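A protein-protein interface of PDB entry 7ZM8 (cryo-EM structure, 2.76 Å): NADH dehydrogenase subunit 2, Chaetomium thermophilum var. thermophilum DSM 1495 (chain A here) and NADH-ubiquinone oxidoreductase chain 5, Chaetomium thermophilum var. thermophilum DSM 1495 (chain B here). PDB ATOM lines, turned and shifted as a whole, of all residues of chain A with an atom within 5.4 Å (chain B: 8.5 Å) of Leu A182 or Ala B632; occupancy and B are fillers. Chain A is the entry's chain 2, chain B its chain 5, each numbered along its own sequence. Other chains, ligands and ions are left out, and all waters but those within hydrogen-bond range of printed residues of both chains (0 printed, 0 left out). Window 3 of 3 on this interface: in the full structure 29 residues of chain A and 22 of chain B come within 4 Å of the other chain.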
ATOM      1  N   LEU A 177       9.819  -8.236  28.902  1.00  0.00           N
ATOM      2  CA  LEU A 177       9.232  -7.769  27.652  1.00  0.00           C
ATOM      3  C   LEU A 177       8.490  -8.897  26.952  1.00  0.00           C
ATOM      4  O   LEU A 177       7.353  -8.723  26.503  1.00  0.00           O
ATOM      5  CB  LEU A 177      10.320  -7.188  26.752  1.00  0.00           C
ATOM      6  CG  LEU A 177       9.883  -6.712  25.371  1.00  0.00           C
ATOM      7  CD1 LEU A 177       9.164  -5.381  25.449  1.00  0.00           C
ATOM      8  CD2 LEU A 177      11.076  -6.614  24.477  1.00  0.00           C
ATOM      9  N   ILE A 178       9.122 -10.069  26.859  1.00  0.00           N
ATOM     10  CA  ILE A 178       8.459 -11.251  26.319  1.00  0.00           C
ATOM     11  C   ILE A 178       7.181 -11.539  27.094  1.00  0.00           C
ATOM     12  O   ILE A 178       6.117 -11.786  26.514  1.00  0.00           O
ATOM     13  CB  ILE A 178       9.417 -12.457  26.355  1.00  0.00           C
ATOM     14  CG1 ILE A 178      10.619 -12.217  25.442  1.00  0.00           C
ATOM     15  CG2 ILE A 178       8.695 -13.747  26.007  1.00  0.00           C
ATOM     16  CD1 ILE A 178      11.802 -13.113  25.733  1.00  0.00           C
ATOM     17  N   TYR A 179       7.247 -11.511  28.427  1.00  0.00           N
ATOM     18  CA  TYR A 179       6.091 -11.839  29.308  1.00  0.00           C
ATOM     19  C   TYR A 179       4.938 -10.844  29.129  1.00  0.00           C
ATOM     20  O   TYR A 179       3.818 -11.281  28.925  1.00  0.00           O
ATOM     21  CB  TYR A 179       6.592 -11.972  30.750  1.00  0.00           C
ATOM     22  CG  TYR A 179       5.697 -12.679  31.736  1.00  0.00           C
ATOM     23  CD1 TYR A 179       4.588 -13.401  31.330  1.00  0.00           C
ATOM     24  CD2 TYR A 179       5.984 -12.640  33.089  1.00  0.00           C
ATOM     25  CE1 TYR A 179       3.777 -14.047  32.246  1.00  0.00           C
ATOM     26  CE2 TYR A 179       5.187 -13.285  34.017  1.00  0.00           C
ATOM     27  CZ  TYR A 179       4.080 -13.994  33.592  1.00  0.00           C
ATOM     28  OH  TYR A 179       3.291 -14.631  34.504  1.00  0.00           O
ATOM     29  N   PHE A 180       5.219  -9.550  29.144  1.00  0.00           N
ATOM     30  CA  PHE A 180       4.165  -8.524  28.969  1.00  0.00           C
ATOM     31  C   PHE A 180       3.505  -8.656  27.613  1.00  0.00           C
ATOM     32  O   PHE A 180       2.292  -8.482  27.514  1.00  0.00           O
ATOM     33  CB  PHE A 180       4.740  -7.109  29.054  1.00  0.00           C
ATOM     34  CG  PHE A 180       3.809  -6.041  28.547  1.00  0.00           C
ATOM     35  CD1 PHE A 180       2.826  -5.519  29.366  1.00  0.00           C
ATOM     36  CD2 PHE A 180       3.896  -5.584  27.242  1.00  0.00           C
ATOM     37  CE1 PHE A 180       1.948  -4.562  28.888  1.00  0.00           C
ATOM     38  CE2 PHE A 180       3.007  -4.641  26.763  1.00  0.00           C
ATOM     39  CZ  PHE A 180       2.036  -4.130  27.586  1.00  0.00           C
ATOM     40  N   LEU A 181       4.275  -8.996  26.596  1.00  0.00           N
ATOM     41  CA  LEU A 181       3.745  -8.974  25.222  1.00  0.00           C
ATOM     42  C   LEU A 181       2.944 -10.232  24.981  1.00  0.00           C
ATOM     43  O   LEU A 181       1.870 -10.127  24.421  1.00  0.00           O
ATOM     44  CB  LEU A 181       4.938  -8.904  24.275  1.00  0.00           C
ATOM     45  CG  LEU A 181       5.338  -7.503  23.829  1.00  0.00           C
ATOM     46  CD1 LEU A 181       6.688  -7.518  23.131  1.00  0.00           C
ATOM     47  CD2 LEU A 181       4.272  -6.925  22.920  1.00  0.00           C
ATOM     48  N   LEU A 182       3.441 -11.371  25.433  1.00  0.00           N
ATOM     49  CA  LEU A 182       2.626 -12.559  25.240  1.00  0.00           C
ATOM     50  C   LEU A 182       1.514 -12.671  26.265  1.00  0.00           C
ATOM     51  O   LEU A 182       0.531 -13.375  26.018  1.00  0.00           O
ATOM     52  CB  LEU A 182       3.506 -13.808  25.278  1.00  0.00           C
ATOM     53  CG  LEU A 182       4.411 -13.997  24.065  1.00  0.00           C
ATOM     54  CD1 LEU A 182       5.265 -15.234  24.219  1.00  0.00           C
ATOM     55  CD2 LEU A 182       3.586 -14.048  22.791  1.00  0.00           C
ATOM     56  N   GLY A 183       1.653 -11.959  27.369  1.00  0.00           N
ATOM     57  CA  GLY A 183       0.661 -11.934  28.452  1.00  0.00           C
ATOM     58  C   GLY A 183      -0.486 -11.027  28.106  1.00  0.00           C
ATOM     59  O   GLY A 183      -1.587 -11.267  28.594  1.00  0.00           O
ATOM     60  N   GLY A 184      -0.201  -9.940  27.403  1.00  0.00           N
ATOM     61  CA  GLY A 184      -1.256  -9.034  26.917  1.00  0.00           C
ATOM     62  C   GLY A 184      -2.150  -9.667  25.878  1.00  0.00           C
ATOM     63  O   GLY A 184      -3.345  -9.377  25.865  1.00  0.00           O
ATOM     64  N   LEU A 185      -1.572 -10.468  25.006  1.00  0.00           N
ATOM     65  CA  LEU A 185      -2.418 -11.170  24.030  1.00  0.00           C
ATOM     66  C   LEU A 185      -3.286 -12.183  24.773  1.00  0.00           C
ATOM     67  O   LEU A 185      -4.420 -12.422  24.337  1.00  0.00           O
ATOM     68  CB  LEU A 185      -1.491 -11.860  23.022  1.00  0.00           C
ATOM     69  CG  LEU A 185      -2.155 -12.614  21.874  1.00  0.00           C
ATOM     70  CD1 LEU A 185      -2.875 -11.657  20.945  1.00  0.00           C
ATOM     71  CD2 LEU A 185      -1.119 -13.417  21.103  1.00  0.00           C
ATOM     72  N   SER A 186      -2.769 -12.751  25.856  1.00  0.00           N
ATOM     73  CA  SER A 186      -3.594 -13.632  26.670  1.00  0.00           C
ATOM     74  C   SER A 186      -4.741 -12.873  27.325  1.00  0.00           C
ATOM     75  O   SER A 186      -5.846 -13.408  27.472  1.00  0.00           O
ATOM     76  CB  SER A 186      -2.722 -14.310  27.723  1.00  0.00           C
ATOM     77  OG  SER A 186      -3.480 -15.155  28.563  1.00  0.00           O
ATOM     78  N   PHE A 253      -2.818 -20.082  28.906  1.00  0.00           N
ATOM     79  CA  PHE A 253      -1.536 -19.423  28.692  1.00  0.00           C
ATOM     80  C   PHE A 253      -0.904 -19.013  30.010  1.00  0.00           C
ATOM     81  O   PHE A 253       0.299 -19.200  30.215  1.00  0.00           O
ATOM     82  CB  PHE A 253      -1.706 -18.203  27.789  1.00  0.00           C
ATOM     83  CG  PHE A 253      -0.445 -17.402  27.629  1.00  0.00           C
ATOM     84  CD1 PHE A 253      -0.107 -16.410  28.539  1.00  0.00           C
ATOM     85  CD2 PHE A 253       0.415 -17.656  26.584  1.00  0.00           C
ATOM     86  CE1 PHE A 253       1.051 -15.697  28.404  1.00  0.00           C
ATOM     87  CE2 PHE A 253       1.568 -16.936  26.440  1.00  0.00           C
ATOM     88  CZ  PHE A 253       1.894 -15.966  27.351  1.00  0.00           C
ATOM     89  N   TRP A 263       6.500 -19.634  26.208  1.00  0.00           N
ATOM     90  CA  TRP A 263       7.050 -18.467  26.884  1.00  0.00           C
ATOM     91  C   TRP A 263       7.757 -18.842  28.180  1.00  0.00           C
ATOM     92  O   TRP A 263       8.797 -18.266  28.509  1.00  0.00           O
ATOM     93  CB  TRP A 263       5.936 -17.461  27.150  1.00  0.00           C
ATOM     94  CG  TRP A 263       4.901 -17.957  28.110  1.00  0.00           C
ATOM     95  CD1 TRP A 263       3.819 -18.721  27.816  1.00  0.00           C
ATOM     96  CD2 TRP A 263       4.857 -17.727  29.520  1.00  0.00           C
ATOM     97  NE1 TRP A 263       3.096 -18.974  28.946  1.00  0.00           N
ATOM     98  CE2 TRP A 263       3.714 -18.375  30.008  1.00  0.00           C
ATOM     99  CE3 TRP A 263       5.675 -17.035  30.417  1.00  0.00           C
ATOM    100  CZ2 TRP A 263       3.364 -18.353  31.353  1.00  0.00           C
ATOM    101  CZ3 TRP A 263       5.337 -17.029  31.745  1.00  0.00           C
ATOM    102  CH2 TRP A 263       4.183 -17.670  32.202  1.00  0.00           C
ATOM    103  N   SER B 626      12.808 -17.913  20.897  1.00  0.00           N
ATOM    104  CA  SER B 626      12.706 -16.723  21.741  1.00  0.00           C
ATOM    105  C   SER B 626      12.394 -15.471  20.927  1.00  0.00           C
ATOM    106  O   SER B 626      12.879 -14.381  21.235  1.00  0.00           O
ATOM    107  CB  SER B 626      13.971 -16.513  22.574  1.00  0.00           C
ATOM    108  OG  SER B 626      14.927 -15.746  21.867  1.00  0.00           O
ATOM    109  N   HIS B 627      11.591 -15.612  19.878  1.00  0.00           N
ATOM    110  CA  HIS B 627      11.052 -14.473  19.153  1.00  0.00           C
ATOM    111  C   HIS B 627       9.604 -14.292  19.571  1.00  0.00           C
ATOM    112  O   HIS B 627       8.799 -15.218  19.444  1.00  0.00           O
ATOM    113  CB  HIS B 627      11.150 -14.659  17.642  1.00  0.00           C
ATOM    114  CG  HIS B 627      12.540 -14.900  17.154  1.00  0.00           C
ATOM    115  ND1 HIS B 627      12.871 -15.972  16.356  1.00  0.00           N
ATOM    116  CD2 HIS B 627      13.687 -14.212  17.356  1.00  0.00           C
ATOM    117  CE1 HIS B 627      14.163 -15.932  16.085  1.00  0.00           C
ATOM    118  NE2 HIS B 627      14.682 -14.875  16.682  1.00  0.00           N
ATOM    119  N   VAL B 628       9.281 -13.108  20.085  1.00  0.00           N
ATOM    120  CA  VAL B 628       7.910 -12.836  20.492  1.00  0.00           C
ATOM    121  C   VAL B 628       6.972 -12.859  19.299  1.00  0.00           C
ATOM    122  O   VAL B 628       5.811 -13.255  19.423  1.00  0.00           O
ATOM    123  CB  VAL B 628       7.845 -11.505  21.266  1.00  0.00           C
ATOM    124  CG1 VAL B 628       8.598 -11.634  22.554  1.00  0.00           C
ATOM    125  CG2 VAL B 628       8.496 -10.421  20.456  1.00  0.00           C
ATOM    126  N   THR B 629       7.448 -12.428  18.132  1.00  0.00           N
ATOM    127  CA  THR B 629       6.609 -12.468  16.942  1.00  0.00           C
ATOM    128  C   THR B 629       6.243 -13.897  16.567  1.00  0.00           C
ATOM    129  O   THR B 629       5.093 -14.171  16.213  1.00  0.00           O
ATOM    130  CB  THR B 629       7.305 -11.755  15.782  1.00  0.00           C
ATOM    131  OG1 THR B 629       8.565 -12.378  15.513  1.00  0.00           O
ATOM    132  CG2 THR B 629       7.514 -10.288  16.095  1.00  0.00           C
ATOM    133  N   THR B 630       7.198 -14.825  16.642  1.00  0.00           N
ATOM    134  CA  THR B 630       6.883 -16.204  16.291  1.00  0.00           C
ATOM    135  C   THR B 630       6.114 -16.917  17.399  1.00  0.00           C
ATOM    136  O   THR B 630       5.336 -17.833  17.111  1.00  0.00           O
ATOM    137  CB  THR B 630       8.154 -16.981  15.928  1.00  0.00           C
ATOM    138  OG1 THR B 630       7.787 -18.194  15.266  1.00  0.00           O
ATOM    139  CG2 THR B 630       8.934 -17.360  17.150  1.00  0.00           C
ATOM    140  N   TYR B 631       6.307 -16.523  18.659  1.00  0.00           N
ATOM    141  CA  TYR B 631       5.531 -17.123  19.738  1.00  0.00           C
ATOM    142  C   TYR B 631       4.077 -16.689  19.669  1.00  0.00           C
ATOM    143  O   TYR B 631       3.172 -17.473  19.970  1.00  0.00           O
ATOM    144  CB  TYR B 631       6.128 -16.751  21.094  1.00  0.00           C
ATOM    145  CG  TYR B 631       7.381 -17.508  21.459  1.00  0.00           C
ATOM    146  CD1 TYR B 631       7.831 -18.564  20.686  1.00  0.00           C
ATOM    147  CD2 TYR B 631       8.115 -17.160  22.579  1.00  0.00           C
ATOM    148  CE1 TYR B 631       8.979 -19.252  21.020  1.00  0.00           C
ATOM    149  CE2 TYR B 631       9.261 -17.841  22.918  1.00  0.00           C
ATOM    150  CZ  TYR B 631       9.687 -18.886  22.136  1.00  0.00           C
ATOM    151  OH  TYR B 631      10.832 -19.558  22.481  1.00  0.00           O
ATOM    152  N   ALA B 632       3.838 -15.435  19.286  1.00  0.00           N
ATOM    153  CA  ALA B 632       2.476 -14.942  19.141  1.00  0.00           C
ATOM    154  C   ALA B 632       1.726 -15.701  18.060  1.00  0.00           C
ATOM    155  O   ALA B 632       0.538 -16.002  18.209  1.00  0.00           O
ATOM    156  CB  ALA B 632       2.504 -13.454  18.825  1.00  0.00           C
ATOM    157  N   LEU B 633       2.409 -16.017  16.961  1.00  0.00           N
ATOM    158  CA  LEU B 633       1.794 -16.799  15.899  1.00  0.00           C
ATOM    159  C   LEU B 633       1.401 -18.181  16.398  1.00  0.00           C
ATOM    160  O   LEU B 633       0.359 -18.717  16.009  1.00  0.00           O
ATOM    161  CB  LEU B 633       2.757 -16.896  14.718  1.00  0.00           C
ATOM    162  CG  LEU B 633       2.175 -17.211  13.346  1.00  0.00           C
ATOM    163  CD1 LEU B 633       1.170 -16.148  12.953  1.00  0.00           C
ATOM    164  CD2 LEU B 633       3.286 -17.304  12.316  1.00  0.00           C
ATOM    165  N   TYR B 634       2.222 -18.770  17.269  1.00  0.00           N
ATOM    166  CA  TYR B 634       1.918 -20.087  17.817  1.00  0.00           C
ATOM    167  C   TYR B 634       0.656 -20.059  18.669  1.00  0.00           C
ATOM    168  O   TYR B 634      -0.162 -20.982  18.604  1.00  0.00           O
ATOM    169  CB  TYR B 634       3.097 -20.598  18.643  1.00  0.00           C
ATOM    170  CG  TYR B 634       4.323 -20.955  17.843  1.00  0.00           C
ATOM    171  CD1 TYR B 634       4.261 -21.102  16.467  1.00  0.00           C
ATOM    172  CD2 TYR B 634       5.544 -21.148  18.466  1.00  0.00           C
ATOM    173  CE1 TYR B 634       5.380 -21.432  15.735  1.00  0.00           C
ATOM    174  CE2 TYR B 634       6.671 -21.482  17.741  1.00  0.00           C
ATOM    175  CZ  TYR B 634       6.581 -21.622  16.376  1.00  0.00           C
ATOM    176  OH  TYR B 634       7.694 -21.946  15.643  1.00  0.00           O
ATOM    177  N   ILE B 635       0.489 -19.016  19.481  1.00  0.00           N
ATOM    178  CA  ILE B 635      -0.698 -18.911  20.327  1.00  0.00           C
ATOM    179  C   ILE B 635      -1.956 -18.818  19.478  1.00  0.00           C
ATOM    180  O   ILE B 635      -2.974 -19.448  19.785  1.00  0.00           O
ATOM    181  CB  ILE B 635      -0.570 -17.717  21.287  1.00  0.00           C
ATOM    182  CG1 ILE B 635       0.606 -17.927  22.235  1.00  0.00           C
ATOM    183  CG2 ILE B 635      -1.856 -17.515  22.061  1.00  0.00           C
ATOM    184  CD1 ILE B 635       0.965 -16.708  23.034  1.00  0.00           C
ATOM    185  N   LEU B 636      -1.914 -18.024  18.405  1.00  0.00           N
ATOM    186  CA  LEU B 636      -3.049 -17.970  17.492  1.00  0.00           C
ATOM    187  C   LEU B 636      -3.305 -19.323  16.850  1.00  0.00           C
ATOM    188  O   LEU B 636      -4.458 -19.745  16.723  1.00  0.00           O
ATOM    189  CB  LEU B 636      -2.819 -16.912  16.417  1.00  0.00           C
ATOM    190  CG  LEU B 636      -3.337 -15.499  16.669  1.00  0.00           C
ATOM    191  CD1 LEU B 636      -4.844 -15.504  16.514  1.00  0.00           C
ATOM    192  CD2 LEU B 636      -2.931 -14.962  18.037  1.00  0.00           C
ATOM    193  N   VAL B 637      -2.244 -20.015  16.437  1.00  0.00           N
ATOM    194  CA  VAL B 637      -2.408 -21.328  15.826  1.00  0.00           C
ATOM    195  C   VAL B 637      -3.060 -22.285  16.810  1.00  0.00           C
ATOM    196  O   VAL B 637      -4.078 -22.916  16.508  1.00  0.00           O
ATOM    197  CB  VAL B 637      -1.052 -21.861  15.335  1.00  0.00           C
ATOM    198  CG1 VAL B 637      -1.146 -23.343  15.011  1.00  0.00           C
ATOM    199  CG2 VAL B 637      -0.588 -21.076  14.128  1.00  0.00           C
ATOM    200  N   GLY B 638      -2.513 -22.371  18.022  1.00  0.00           N
ATOM    201  CA  GLY B 638      -3.099 -23.221  19.041  1.00  0.00           C
ATOM    202  C   GLY B 638      -4.472 -22.776  19.479  1.00  0.00           C
ATOM    203  O   GLY B 638      -5.242 -23.590  19.996  1.00  0.00           O
ATOM    204  N   PHE B 639      -4.790 -21.493  19.299  1.00  0.00           N
ATOM    205  CA  PHE B 639      -6.146 -21.020  19.542  1.00  0.00           C
ATOM    206  C   PHE B 639      -7.114 -21.544  18.491  1.00  0.00           C
ATOM    207  O   PHE B 639      -8.193 -22.038  18.825  1.00  0.00           O
ATOM    208  CB  PHE B 639      -6.157 -19.494  19.575  1.00  0.00           C
ATOM    209  CG  PHE B 639      -7.503 -18.899  19.859  1.00  0.00           C
ATOM    210  CD1 PHE B 639      -8.026 -18.910  21.140  1.00  0.00           C
ATOM    211  CD2 PHE B 639      -8.241 -18.312  18.843  1.00  0.00           C
ATOM    212  CE1 PHE B 639      -9.266 -18.356  21.403  1.00  0.00           C
ATOM    213  CE2 PHE B 639      -9.477 -17.761  19.100  1.00  0.00           C
ATOM    214  CZ  PHE B 639      -9.990 -17.779  20.380  1.00  0.00           C
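The backbone carbonyl oxygen (O) of Phe A253 is in hydrogen-bond range of the indole nitrogen (NE1) of Trp A263, at 3.1 Å.
N of Ser B626 is in hydrogen-bond range of OH of Tyr B631, 3.0 Å away.
Of the printed residues of chain B, Leu A182 touches Tyr B631, Ala B632 and Ile B635.
Of chain A, only Leu A182 comes within 4 Å of Ala B632.
Of the printed residues of chain B, Phe A253 touches Ile B635.
Printed residues of chain B within 4 Å of Leu A185: Leu B636.
Of the printed residues of chain B, Ile A178 touches Val B628 (3.6 Å).
Ser B626 touches none of the printed residues of chain A.
The nearest residue of chain A that does not touch Ala B632 is Leu A185 (4.2 Å).
The nearest printed residue of chain A that does not touch Leu B636 is Leu A182 (8.1 Å).
Printed residues of chain B that touch a printed residue of chain A: Val B628, Tyr B631, Ala B632, Ile B635 and Leu B636.
Among the printed residues, 6 pairs touch across the chains.
Among the printed residues, no Asp or Glu carboxylate lies within 4 Å of a Lys or Arg side-chain nitrogen of the other chain.
Among the printed residues, merely in contact across the chains: Ile A178 with Val B628 (3.6 Å), Leu A182 with Tyr B631 (3.6 Å), Leu A182 with Ala B632 (3.8 Å), Leu A182 with Ile B635 (3.7 Å), Leu A185 with Leu B636 (3.9 Å) and Phe A253 with Ile B635 (3.5 Å).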
